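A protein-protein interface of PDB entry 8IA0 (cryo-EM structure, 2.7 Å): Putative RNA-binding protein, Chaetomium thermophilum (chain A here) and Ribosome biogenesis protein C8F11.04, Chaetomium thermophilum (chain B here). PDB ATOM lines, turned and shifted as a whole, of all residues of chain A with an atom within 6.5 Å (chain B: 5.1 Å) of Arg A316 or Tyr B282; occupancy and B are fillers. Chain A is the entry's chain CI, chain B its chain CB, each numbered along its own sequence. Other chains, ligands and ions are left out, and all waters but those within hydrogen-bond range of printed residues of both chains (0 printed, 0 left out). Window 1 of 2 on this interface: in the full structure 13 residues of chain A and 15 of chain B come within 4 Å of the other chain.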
ATOM      1  N   GLU A 309     -29.582 -37.463 -27.234  1.00  0.00           N
ATOM      2  CA  GLU A 309     -29.259 -36.041 -27.236  1.00  0.00           C
ATOM      3  C   GLU A 309     -28.897 -35.566 -25.835  1.00  0.00           C
ATOM      4  O   GLU A 309     -27.959 -34.778 -25.665  1.00  0.00           O
ATOM      5  CB  GLU A 309     -30.428 -35.231 -27.798  1.00  0.00           C
ATOM      6  CG  GLU A 309     -30.583 -35.327 -29.307  1.00  0.00           C
ATOM      7  CD  GLU A 309     -29.430 -34.684 -30.055  1.00  0.00           C
ATOM      8  OE1 GLU A 309     -28.866 -33.693 -29.543  1.00  0.00           O
ATOM      9  OE2 GLU A 309     -29.089 -35.168 -31.153  1.00  0.00           O
ATOM     10  N   GLN A 311     -27.575 -37.390 -23.402  1.00  0.00           N
ATOM     11  CA  GLN A 311     -26.245 -37.886 -23.069  1.00  0.00           C
ATOM     12  C   GLN A 311     -25.168 -37.153 -23.858  1.00  0.00           C
ATOM     13  O   GLN A 311     -24.062 -36.942 -23.347  1.00  0.00           O
ATOM     14  CB  GLN A 311     -26.161 -39.399 -23.296  1.00  0.00           C
ATOM     15  CG  GLN A 311     -26.017 -39.831 -24.743  1.00  0.00           C
ATOM     16  CD  GLN A 311     -26.020 -41.337 -24.905  1.00  0.00           C
ATOM     17  OE1 GLN A 311     -26.078 -42.079 -23.925  1.00  0.00           O
ATOM     18  NE2 GLN A 311     -25.956 -41.798 -26.149  1.00  0.00           N
ATOM     19  N   ARG A 312     -25.467 -36.757 -25.099  1.00  0.00           N
ATOM     20  CA  ARG A 312     -24.558 -35.879 -25.828  1.00  0.00           C
ATOM     21  C   ARG A 312     -24.437 -34.530 -25.133  1.00  0.00           C
ATOM     22  O   ARG A 312     -23.340 -33.970 -25.034  1.00  0.00           O
ATOM     23  CB  ARG A 312     -25.035 -35.702 -27.269  1.00  0.00           C
ATOM     24  CG  ARG A 312     -23.980 -35.131 -28.199  1.00  0.00           C
ATOM     25  CD  ARG A 312     -24.342 -35.364 -29.654  1.00  0.00           C
ATOM     26  NE  ARG A 312     -25.435 -34.501 -30.083  1.00  0.00           N
ATOM     27  CZ  ARG A 312     -25.695 -34.195 -31.347  1.00  0.00           C
ATOM     28  NH1 ARG A 312     -24.958 -34.668 -32.338  1.00  0.00           N
ATOM     29  NH2 ARG A 312     -26.719 -33.394 -31.623  1.00  0.00           N
ATOM     30  N   ARG A 313     -25.561 -33.995 -24.650  1.00  0.00           N
ATOM     31  CA  ARG A 313     -25.515 -32.772 -23.856  1.00  0.00           C
ATOM     32  C   ARG A 313     -24.701 -32.967 -22.587  1.00  0.00           C
ATOM     33  O   ARG A 313     -23.983 -32.053 -22.165  1.00  0.00           O
ATOM     34  CB  ARG A 313     -26.931 -32.314 -23.512  1.00  0.00           C
ATOM     35  CG  ARG A 313     -27.719 -31.800 -24.698  1.00  0.00           C
ATOM     36  CD  ARG A 313     -29.084 -31.296 -24.271  1.00  0.00           C
ATOM     37  NE  ARG A 313     -29.859 -30.814 -25.406  1.00  0.00           N
ATOM     38  CZ  ARG A 313     -31.037 -30.213 -25.311  1.00  0.00           C
ATOM     39  NH1 ARG A 313     -31.606 -29.988 -24.137  1.00  0.00           N
ATOM     40  NH2 ARG A 313     -31.659 -29.826 -26.420  1.00  0.00           N
ATOM     41  N   ALA A 314     -24.804 -34.143 -21.962  1.00  0.00           N
ATOM     42  CA  ALA A 314     -23.971 -34.435 -20.801  1.00  0.00           C
ATOM     43  C   ALA A 314     -22.495 -34.437 -21.175  1.00  0.00           C
ATOM     44  O   ALA A 314     -21.660 -33.903 -20.435  1.00  0.00           O
ATOM     45  CB  ALA A 314     -24.375 -35.775 -20.186  1.00  0.00           C
ATOM     46  N   ALA A 315     -22.155 -35.035 -22.319  1.00  0.00           N
ATOM     47  CA  ALA A 315     -20.774 -34.997 -22.788  1.00  0.00           C
ATOM     48  C   ALA A 315     -20.336 -33.569 -23.083  1.00  0.00           C
ATOM     49  O   ALA A 315     -19.209 -33.177 -22.758  1.00  0.00           O
ATOM     50  CB  ALA A 315     -20.615 -35.878 -24.028  1.00  0.00           C
ATOM     51  N   ARG A 316     -21.214 -32.778 -23.702  1.00  0.00           N
ATOM     52  CA  ARG A 316     -20.915 -31.366 -23.914  1.00  0.00           C
ATOM     53  C   ARG A 316     -20.789 -30.631 -22.587  1.00  0.00           C
ATOM     54  O   ARG A 316     -19.963 -29.722 -22.446  1.00  0.00           O
ATOM     55  CB  ARG A 316     -21.992 -30.728 -24.792  1.00  0.00           C
ATOM     56  CG  ARG A 316     -21.878 -29.219 -24.920  1.00  0.00           C
ATOM     57  CD  ARG A 316     -23.220 -28.592 -25.249  1.00  0.00           C
ATOM     58  NE  ARG A 316     -23.937 -29.334 -26.280  1.00  0.00           N
ATOM     59  CZ  ARG A 316     -23.834 -29.096 -27.580  1.00  0.00           C
ATOM     60  NH1 ARG A 316     -23.055 -28.134 -28.047  1.00  0.00           N
ATOM     61  NH2 ARG A 316     -24.532 -29.840 -28.432  1.00  0.00           N
ATOM     62  N   ALA A 317     -21.601 -31.017 -21.598  1.00  0.00           N
ATOM     63  CA  ALA A 317     -21.495 -30.413 -20.274  1.00  0.00           C
ATOM     64  C   ALA A 317     -20.121 -30.663 -19.666  1.00  0.00           C
ATOM     65  O   ALA A 317     -19.557 -29.779 -19.010  1.00  0.00           O
ATOM     66  CB  ALA A 317     -22.596 -30.949 -19.361  1.00  0.00           C
ATOM     67  N   GLU A 318     -19.569 -31.862 -19.867  1.00  0.00           N
ATOM     68  CA  GLU A 318     -18.198 -32.118 -19.443  1.00  0.00           C
ATOM     69  C   GLU A 318     -17.221 -31.228 -20.199  1.00  0.00           C
ATOM     70  O   GLU A 318     -16.245 -30.732 -19.624  1.00  0.00           O
ATOM     71  CB  GLU A 318     -17.847 -33.593 -19.643  1.00  0.00           C
ATOM     72  CG  GLU A 318     -18.868 -34.565 -19.079  1.00  0.00           C
ATOM     73  CD  GLU A 318     -19.409 -34.126 -17.732  1.00  0.00           C
ATOM     74  OE1 GLU A 318     -18.620 -34.062 -16.764  1.00  0.00           O
ATOM     75  OE2 GLU A 318     -20.622 -33.845 -17.639  1.00  0.00           O
ATOM     76  N   LYS A 319     -17.467 -31.014 -21.493  1.00  0.00           N
ATOM     77  CA  LYS A 319     -16.631 -30.101 -22.262  1.00  0.00           C
ATOM     78  C   LYS A 319     -16.811 -28.660 -21.802  1.00  0.00           C
ATOM     79  O   LYS A 319     -15.954 -27.809 -22.066  1.00  0.00           O
ATOM     80  CB  LYS A 319     -16.945 -30.240 -23.754  1.00  0.00           C
ATOM     81  CG  LYS A 319     -16.006 -29.477 -24.677  1.00  0.00           C
ATOM     82  CD  LYS A 319     -16.233 -29.856 -26.130  1.00  0.00           C
ATOM     83  CE  LYS A 319     -17.570 -29.339 -26.634  1.00  0.00           C
ATOM     84  NZ  LYS A 319     -17.751 -29.604 -28.089  1.00  0.00           N
ATOM     85  N   LEU A 320     -17.913 -28.365 -21.110  1.00  0.00           N
ATOM     86  CA  LEU A 320     -18.131 -27.033 -20.563  1.00  0.00           C
ATOM     87  C   LEU A 320     -17.701 -26.908 -19.107  1.00  0.00           C
ATOM     88  O   LEU A 320     -17.894 -25.841 -18.512  1.00  0.00           O
ATOM     89  CB  LEU A 320     -19.605 -26.645 -20.698  1.00  0.00           C
ATOM     90  CG  LEU A 320     -20.122 -26.462 -22.126  1.00  0.00           C
ATOM     91  CD1 LEU A 320     -21.614 -26.167 -22.127  1.00  0.00           C
ATOM     92  CD2 LEU A 320     -19.352 -25.360 -22.838  1.00  0.00           C
ATOM     93  N   LYS A 321     -17.137 -27.964 -18.514  1.00  0.00           N
ATOM     94  CA  LYS A 321     -16.664 -27.866 -17.138  1.00  0.00           C
ATOM     95  C   LYS A 321     -15.425 -26.985 -17.043  1.00  0.00           C
ATOM     96  O   LYS A 321     -15.336 -26.118 -16.166  1.00  0.00           O
ATOM     97  CB  LYS A 321     -16.380 -29.258 -16.576  1.00  0.00           C
ATOM     98  CG  LYS A 321     -17.622 -30.113 -16.357  1.00  0.00           C
ATOM     99  CD  LYS A 321     -18.480 -29.578 -15.218  1.00  0.00           C
ATOM    100  CE  LYS A 321     -19.762 -28.936 -15.732  1.00  0.00           C
ATOM    101  NZ  LYS A 321     -20.626 -28.451 -14.620  1.00  0.00           N
ATOM    102  N   GLU A 322     -14.455 -27.195 -17.935  1.00  0.00           N
ATOM    103  CA  GLU A 322     -13.305 -26.299 -17.994  1.00  0.00           C
ATOM    104  C   GLU A 322     -13.723 -24.890 -18.388  1.00  0.00           C
ATOM    105  O   GLU A 322     -13.118 -23.912 -17.933  1.00  0.00           O
ATOM    106  CB  GLU A 322     -12.249 -26.837 -18.965  1.00  0.00           C
ATOM    107  CG  GLU A 322     -12.098 -28.361 -19.018  1.00  0.00           C
ATOM    108  CD  GLU A 322     -13.183 -29.062 -19.820  1.00  0.00           C
ATOM    109  OE1 GLU A 322     -14.269 -28.475 -20.006  1.00  0.00           O
ATOM    110  OE2 GLU A 322     -12.947 -30.205 -20.266  1.00  0.00           O
ATOM    111  N   TRP B  63     -19.300 -15.754 -32.972  1.00  0.00           N
ATOM    112  CA  TRP B  63     -20.475 -16.091 -33.756  1.00  0.00           C
ATOM    113  C   TRP B  63     -21.557 -16.676 -32.860  1.00  0.00           C
ATOM    114  O   TRP B  63     -21.276 -17.312 -31.840  1.00  0.00           O
ATOM    115  CB  TRP B  63     -20.146 -17.098 -34.868  1.00  0.00           C
ATOM    116  CG  TRP B  63     -18.900 -16.799 -35.645  1.00  0.00           C
ATOM    117  CD1 TRP B  63     -17.613 -16.950 -35.224  1.00  0.00           C
ATOM    118  CD2 TRP B  63     -18.826 -16.328 -36.996  1.00  0.00           C
ATOM    119  NE1 TRP B  63     -16.742 -16.586 -36.221  1.00  0.00           N
ATOM    120  CE2 TRP B  63     -17.462 -16.202 -37.320  1.00  0.00           C
ATOM    121  CE3 TRP B  63     -19.781 -15.993 -37.960  1.00  0.00           C
ATOM    122  CZ2 TRP B  63     -17.030 -15.755 -38.567  1.00  0.00           C
ATOM    123  CZ3 TRP B  63     -19.350 -15.551 -39.195  1.00  0.00           C
ATOM    124  CH2 TRP B  63     -17.988 -15.436 -39.487  1.00  0.00           C
ATOM    125  N   LEU B  64     -22.805 -16.451 -33.258  1.00  0.00           N
ATOM    126  CA  LEU B  64     -23.953 -17.132 -32.678  1.00  0.00           C
ATOM    127  C   LEU B  64     -24.529 -18.049 -33.746  1.00  0.00           C
ATOM    128  O   LEU B  64     -24.784 -17.612 -34.874  1.00  0.00           O
ATOM    129  CB  LEU B  64     -24.995 -16.127 -32.161  1.00  0.00           C
ATOM    130  CG  LEU B  64     -26.059 -15.495 -33.064  1.00  0.00           C
ATOM    131  CD1 LEU B  64     -27.327 -16.338 -33.116  1.00  0.00           C
ATOM    132  CD2 LEU B  64     -26.370 -14.077 -32.615  1.00  0.00           C
ATOM    133  N   THR B  65     -24.697 -19.322 -33.409  1.00  0.00           N
ATOM    134  CA  THR B  65     -25.114 -20.331 -34.375  1.00  0.00           C
ATOM    135  C   THR B  65     -26.566 -20.693 -34.102  1.00  0.00           C
ATOM    136  O   THR B  65     -26.885 -21.276 -33.061  1.00  0.00           O
ATOM    137  CB  THR B  65     -24.220 -21.567 -34.314  1.00  0.00           C
ATOM    138  OG1 THR B  65     -24.733 -22.489 -33.346  1.00  0.00           O
ATOM    139  CG2 THR B  65     -22.802 -21.179 -33.944  1.00  0.00           C
ATOM    140  N   THR B  67     -29.788 -22.873 -34.823  1.00  0.00           N
ATOM    141  CA  THR B  67     -30.173 -24.200 -35.281  1.00  0.00           C
ATOM    142  C   THR B  67     -31.692 -24.245 -35.377  1.00  0.00           C
ATOM    143  O   THR B  67     -32.384 -23.724 -34.496  1.00  0.00           O
ATOM    144  CB  THR B  67     -29.653 -25.278 -34.328  1.00  0.00           C
ATOM    145  OG1 THR B  67     -28.224 -25.340 -34.411  1.00  0.00           O
ATOM    146  CG2 THR B  67     -30.231 -26.635 -34.689  1.00  0.00           C
ATOM    147  N   ASN B 280     -31.891 -24.766 -30.713  1.00  0.00           N
ATOM    148  CA  ASN B 280     -30.713 -24.386 -29.942  1.00  0.00           C
ATOM    149  C   ASN B 280     -30.000 -23.165 -30.521  1.00  0.00           C
ATOM    150  O   ASN B 280     -29.919 -22.975 -31.738  1.00  0.00           O
ATOM    151  CB  ASN B 280     -29.740 -25.561 -29.881  1.00  0.00           C
ATOM    152  CG  ASN B 280     -30.395 -26.832 -29.382  1.00  0.00           C
ATOM    153  OD1 ASN B 280     -30.622 -27.769 -30.148  1.00  0.00           O
ATOM    154  ND2 ASN B 280     -30.702 -26.871 -28.091  1.00  0.00           N
ATOM    155  N   PHE B 281     -29.473 -22.337 -29.619  1.00  0.00           N
ATOM    156  CA  PHE B 281     -28.796 -21.080 -29.940  1.00  0.00           C
ATOM    157  C   PHE B 281     -27.397 -21.160 -29.335  1.00  0.00           C
ATOM    158  O   PHE B 281     -27.216 -20.891 -28.144  1.00  0.00           O
ATOM    159  CB  PHE B 281     -29.574 -19.897 -29.371  1.00  0.00           C
ATOM    160  CG  PHE B 281     -30.529 -19.269 -30.335  1.00  0.00           C
ATOM    161  CD1 PHE B 281     -30.261 -19.242 -31.689  1.00  0.00           C
ATOM    162  CD2 PHE B 281     -31.686 -18.665 -29.874  1.00  0.00           C
ATOM    163  CE1 PHE B 281     -31.144 -18.648 -32.567  1.00  0.00           C
ATOM    164  CE2 PHE B 281     -32.575 -18.079 -30.749  1.00  0.00           C
ATOM    165  CZ  PHE B 281     -32.301 -18.065 -32.096  1.00  0.00           C
ATOM    166  N   TYR B 282     -26.407 -21.521 -30.142  1.00  0.00           N
ATOM    167  CA  TYR B 282     -25.060 -21.789 -29.653  1.00  0.00           C
ATOM    168  C   TYR B 282     -24.160 -20.593 -29.937  1.00  0.00           C
ATOM    169  O   TYR B 282     -24.119 -20.097 -31.068  1.00  0.00           O
ATOM    170  CB  TYR B 282     -24.485 -23.048 -30.303  1.00  0.00           C
ATOM    171  CG  TYR B 282     -25.199 -24.330 -29.942  1.00  0.00           C
ATOM    172  CD1 TYR B 282     -25.966 -24.421 -28.793  1.00  0.00           C
ATOM    173  CD2 TYR B 282     -25.107 -25.447 -30.758  1.00  0.00           C
ATOM    174  CE1 TYR B 282     -26.616 -25.592 -28.459  1.00  0.00           C
ATOM    175  CE2 TYR B 282     -25.756 -26.621 -30.437  1.00  0.00           C
ATOM    176  CZ  TYR B 282     -26.510 -26.690 -29.286  1.00  0.00           C
ATOM    177  OH  TYR B 282     -27.159 -27.859 -28.961  1.00  0.00           O
ATOM    178  N   VAL B 283     -23.444 -20.135 -28.915  1.00  0.00           N
ATOM    179  CA  VAL B 283     -22.432 -19.101 -29.091  1.00  0.00           C
ATOM    180  C   VAL B 283     -21.101 -19.785 -29.369  1.00  0.00           C
ATOM    181  O   VAL B 283     -20.630 -20.598 -28.566  1.00  0.00           O
ATOM    182  CB  VAL B 283     -22.342 -18.194 -27.857  1.00  0.00           C
ATOM    183  CG1 VAL B 283     -21.088 -17.341 -27.918  1.00  0.00           C
ATOM    184  CG2 VAL B 283     -23.580 -17.323 -27.752  1.00  0.00           C
ATOM    185  N   LYS B 284     -20.488 -19.455 -30.502  1.00  0.00           N
ATOM    186  CA  LYS B 284     -19.333 -20.180 -31.008  1.00  0.00           C
ATOM    187  C   LYS B 284     -18.153 -19.239 -31.177  1.00  0.00           C
ATOM    188  O   LYS B 284     -18.300 -18.146 -31.734  1.00  0.00           O
ATOM    189  CB  LYS B 284     -19.661 -20.849 -32.348  1.00  0.00           C
ATOM    190  CG  LYS B 284     -18.542 -21.684 -32.944  1.00  0.00           C
ATOM    191  CD  LYS B 284     -18.031 -22.723 -31.969  1.00  0.00           C
ATOM    192  CE  LYS B 284     -17.392 -23.884 -32.711  1.00  0.00           C
ATOM    193  NZ  LYS B 284     -16.733 -24.841 -31.785  1.00  0.00           N
ATOM    194  N   ALA B 290     -18.999 -24.576 -28.367  1.00  0.00           N
ATOM    195  CA  ALA B 290     -20.279 -23.887 -28.460  1.00  0.00           C
ATOM    196  C   ALA B 290     -20.897 -23.731 -27.079  1.00  0.00           C
ATOM    197  O   ALA B 290     -20.690 -24.570 -26.197  1.00  0.00           O
ATOM    198  CB  ALA B 290     -21.242 -24.641 -29.380  1.00  0.00           C
ATOM    199  N   LEU B 291     -21.657 -22.655 -26.896  1.00  0.00           N
ATOM    200  CA  LEU B 291     -22.299 -22.363 -25.618  1.00  0.00           C
ATOM    201  C   LEU B 291     -23.813 -22.446 -25.764  1.00  0.00           C
ATOM    202  O   LEU B 291     -24.421 -21.553 -26.374  1.00  0.00           O
ATOM    203  CB  LEU B 291     -21.883 -20.980 -25.117  1.00  0.00           C
ATOM    204  CG  LEU B 291     -20.376 -20.813 -24.915  1.00  0.00           C
ATOM    205  CD1 LEU B 291     -20.031 -19.370 -24.602  1.00  0.00           C
ATOM    206  CD2 LEU B 291     -19.875 -21.740 -23.817  1.00  0.00           C
ATOM    207  N   PRO B 292     -24.454 -23.492 -25.244  1.00  0.00           N
ATOM    208  CA  PRO B 292     -25.892 -23.672 -25.469  1.00  0.00           C
ATOM    209  C   PRO B 292     -26.739 -22.531 -24.925  1.00  0.00           C
ATOM    210  O   PRO B 292     -26.477 -21.982 -23.852  1.00  0.00           O
ATOM    211  CB  PRO B 292     -26.216 -24.974 -24.725  1.00  0.00           C
ATOM    212  CG  PRO B 292     -24.916 -25.607 -24.383  1.00  0.00           C
ATOM    213  CD  PRO B 292     -23.789 -24.731 -24.814  1.00  0.00           C
ATOM    214  N   ILE B 293     -27.772 -22.184 -25.694  1.00  0.00           N
ATOM    215  CA  ILE B 293     -28.903 -21.377 -25.241  1.00  0.00           C
ATOM    216  C   ILE B 293     -30.139 -21.959 -25.918  1.00  0.00           C
ATOM    217  O   ILE B 293     -30.332 -21.772 -27.123  1.00  0.00           O
ATOM    218  CB  ILE B 293     -28.763 -19.884 -25.581  1.00  0.00           C
ATOM    219  CG1 ILE B 293     -27.406 -19.331 -25.141  1.00  0.00           C
ATOM    220  CG2 ILE B 293     -29.890 -19.089 -24.942  1.00  0.00           C
ATOM    221  CD1 ILE B 293     -27.100 -17.958 -25.693  1.00  0.00           C
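The guanidinium group (NH2) of Arg A316 is in hydrogen-bond range of the side-chain hydroxyl (OH) of Tyr B282 (3.3 Å).
The backbone carbonyl oxygen (O) of Val B283 lies within hydrogen-bond range of the backbone NH (N) of Leu B291, at 2.8 Å. The backbone NH (N) of Thr B65 is in hydrogen-bond range of the backbone carbonyl oxygen (O) of Tyr B282, at 2.5 Å. N of Thr B67 sits at hydrogen-bond distance from O of Asn B280.
Among the printed residues, pairs that only touch across the chains: Arg A313 with Asn B280, Arg A316 with Pro B292, Leu A320 with Ala B290, Leu A320 with Pro B292 and Leu A320 with Leu B291.
Printed residues of chain B within 4 Å of Arg A313: Asn B280. Arg A316 touches just these residues of chain B: Tyr B282 (3.3 Å) and Pro B292 (3.5 Å). Printed residues of chain A within 4 Å of Tyr B282: Arg A316. Lys B284 touches none of the printed residues of chain A. Of the printed residues of chain A, Leu B291 touches Leu A320 (3.8 Å). Of the printed residues of chain A, Pro B292 touches Arg A316 and Leu A320. Ile B293 touches none of the printed residues of chain A. The nearest residue of chain A that does not touch Tyr B282 is Arg A313 (5.4 Å). The nearest printed residue of chain A that does not touch Leu B291 is Arg A316 (5.8 Å).
Printed residues of chain B that touch a printed residue of chain A: Asn B280, Tyr B282, Ala B290, Leu B291 and Pro B292. Hydrophobic or aromatic side chains of chain B within 4 Å of the printed part of chain A: Tyr B282, Leu B291 and Pro B292. Hydrophobic or aromatic side chains of chain A that line the printed part of chain B: Leu A320. Along chain A the printed residues that touch a printed residue of chain B span positions 313 to 320. Among the printed residues, 6 pairs touch across the chains.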
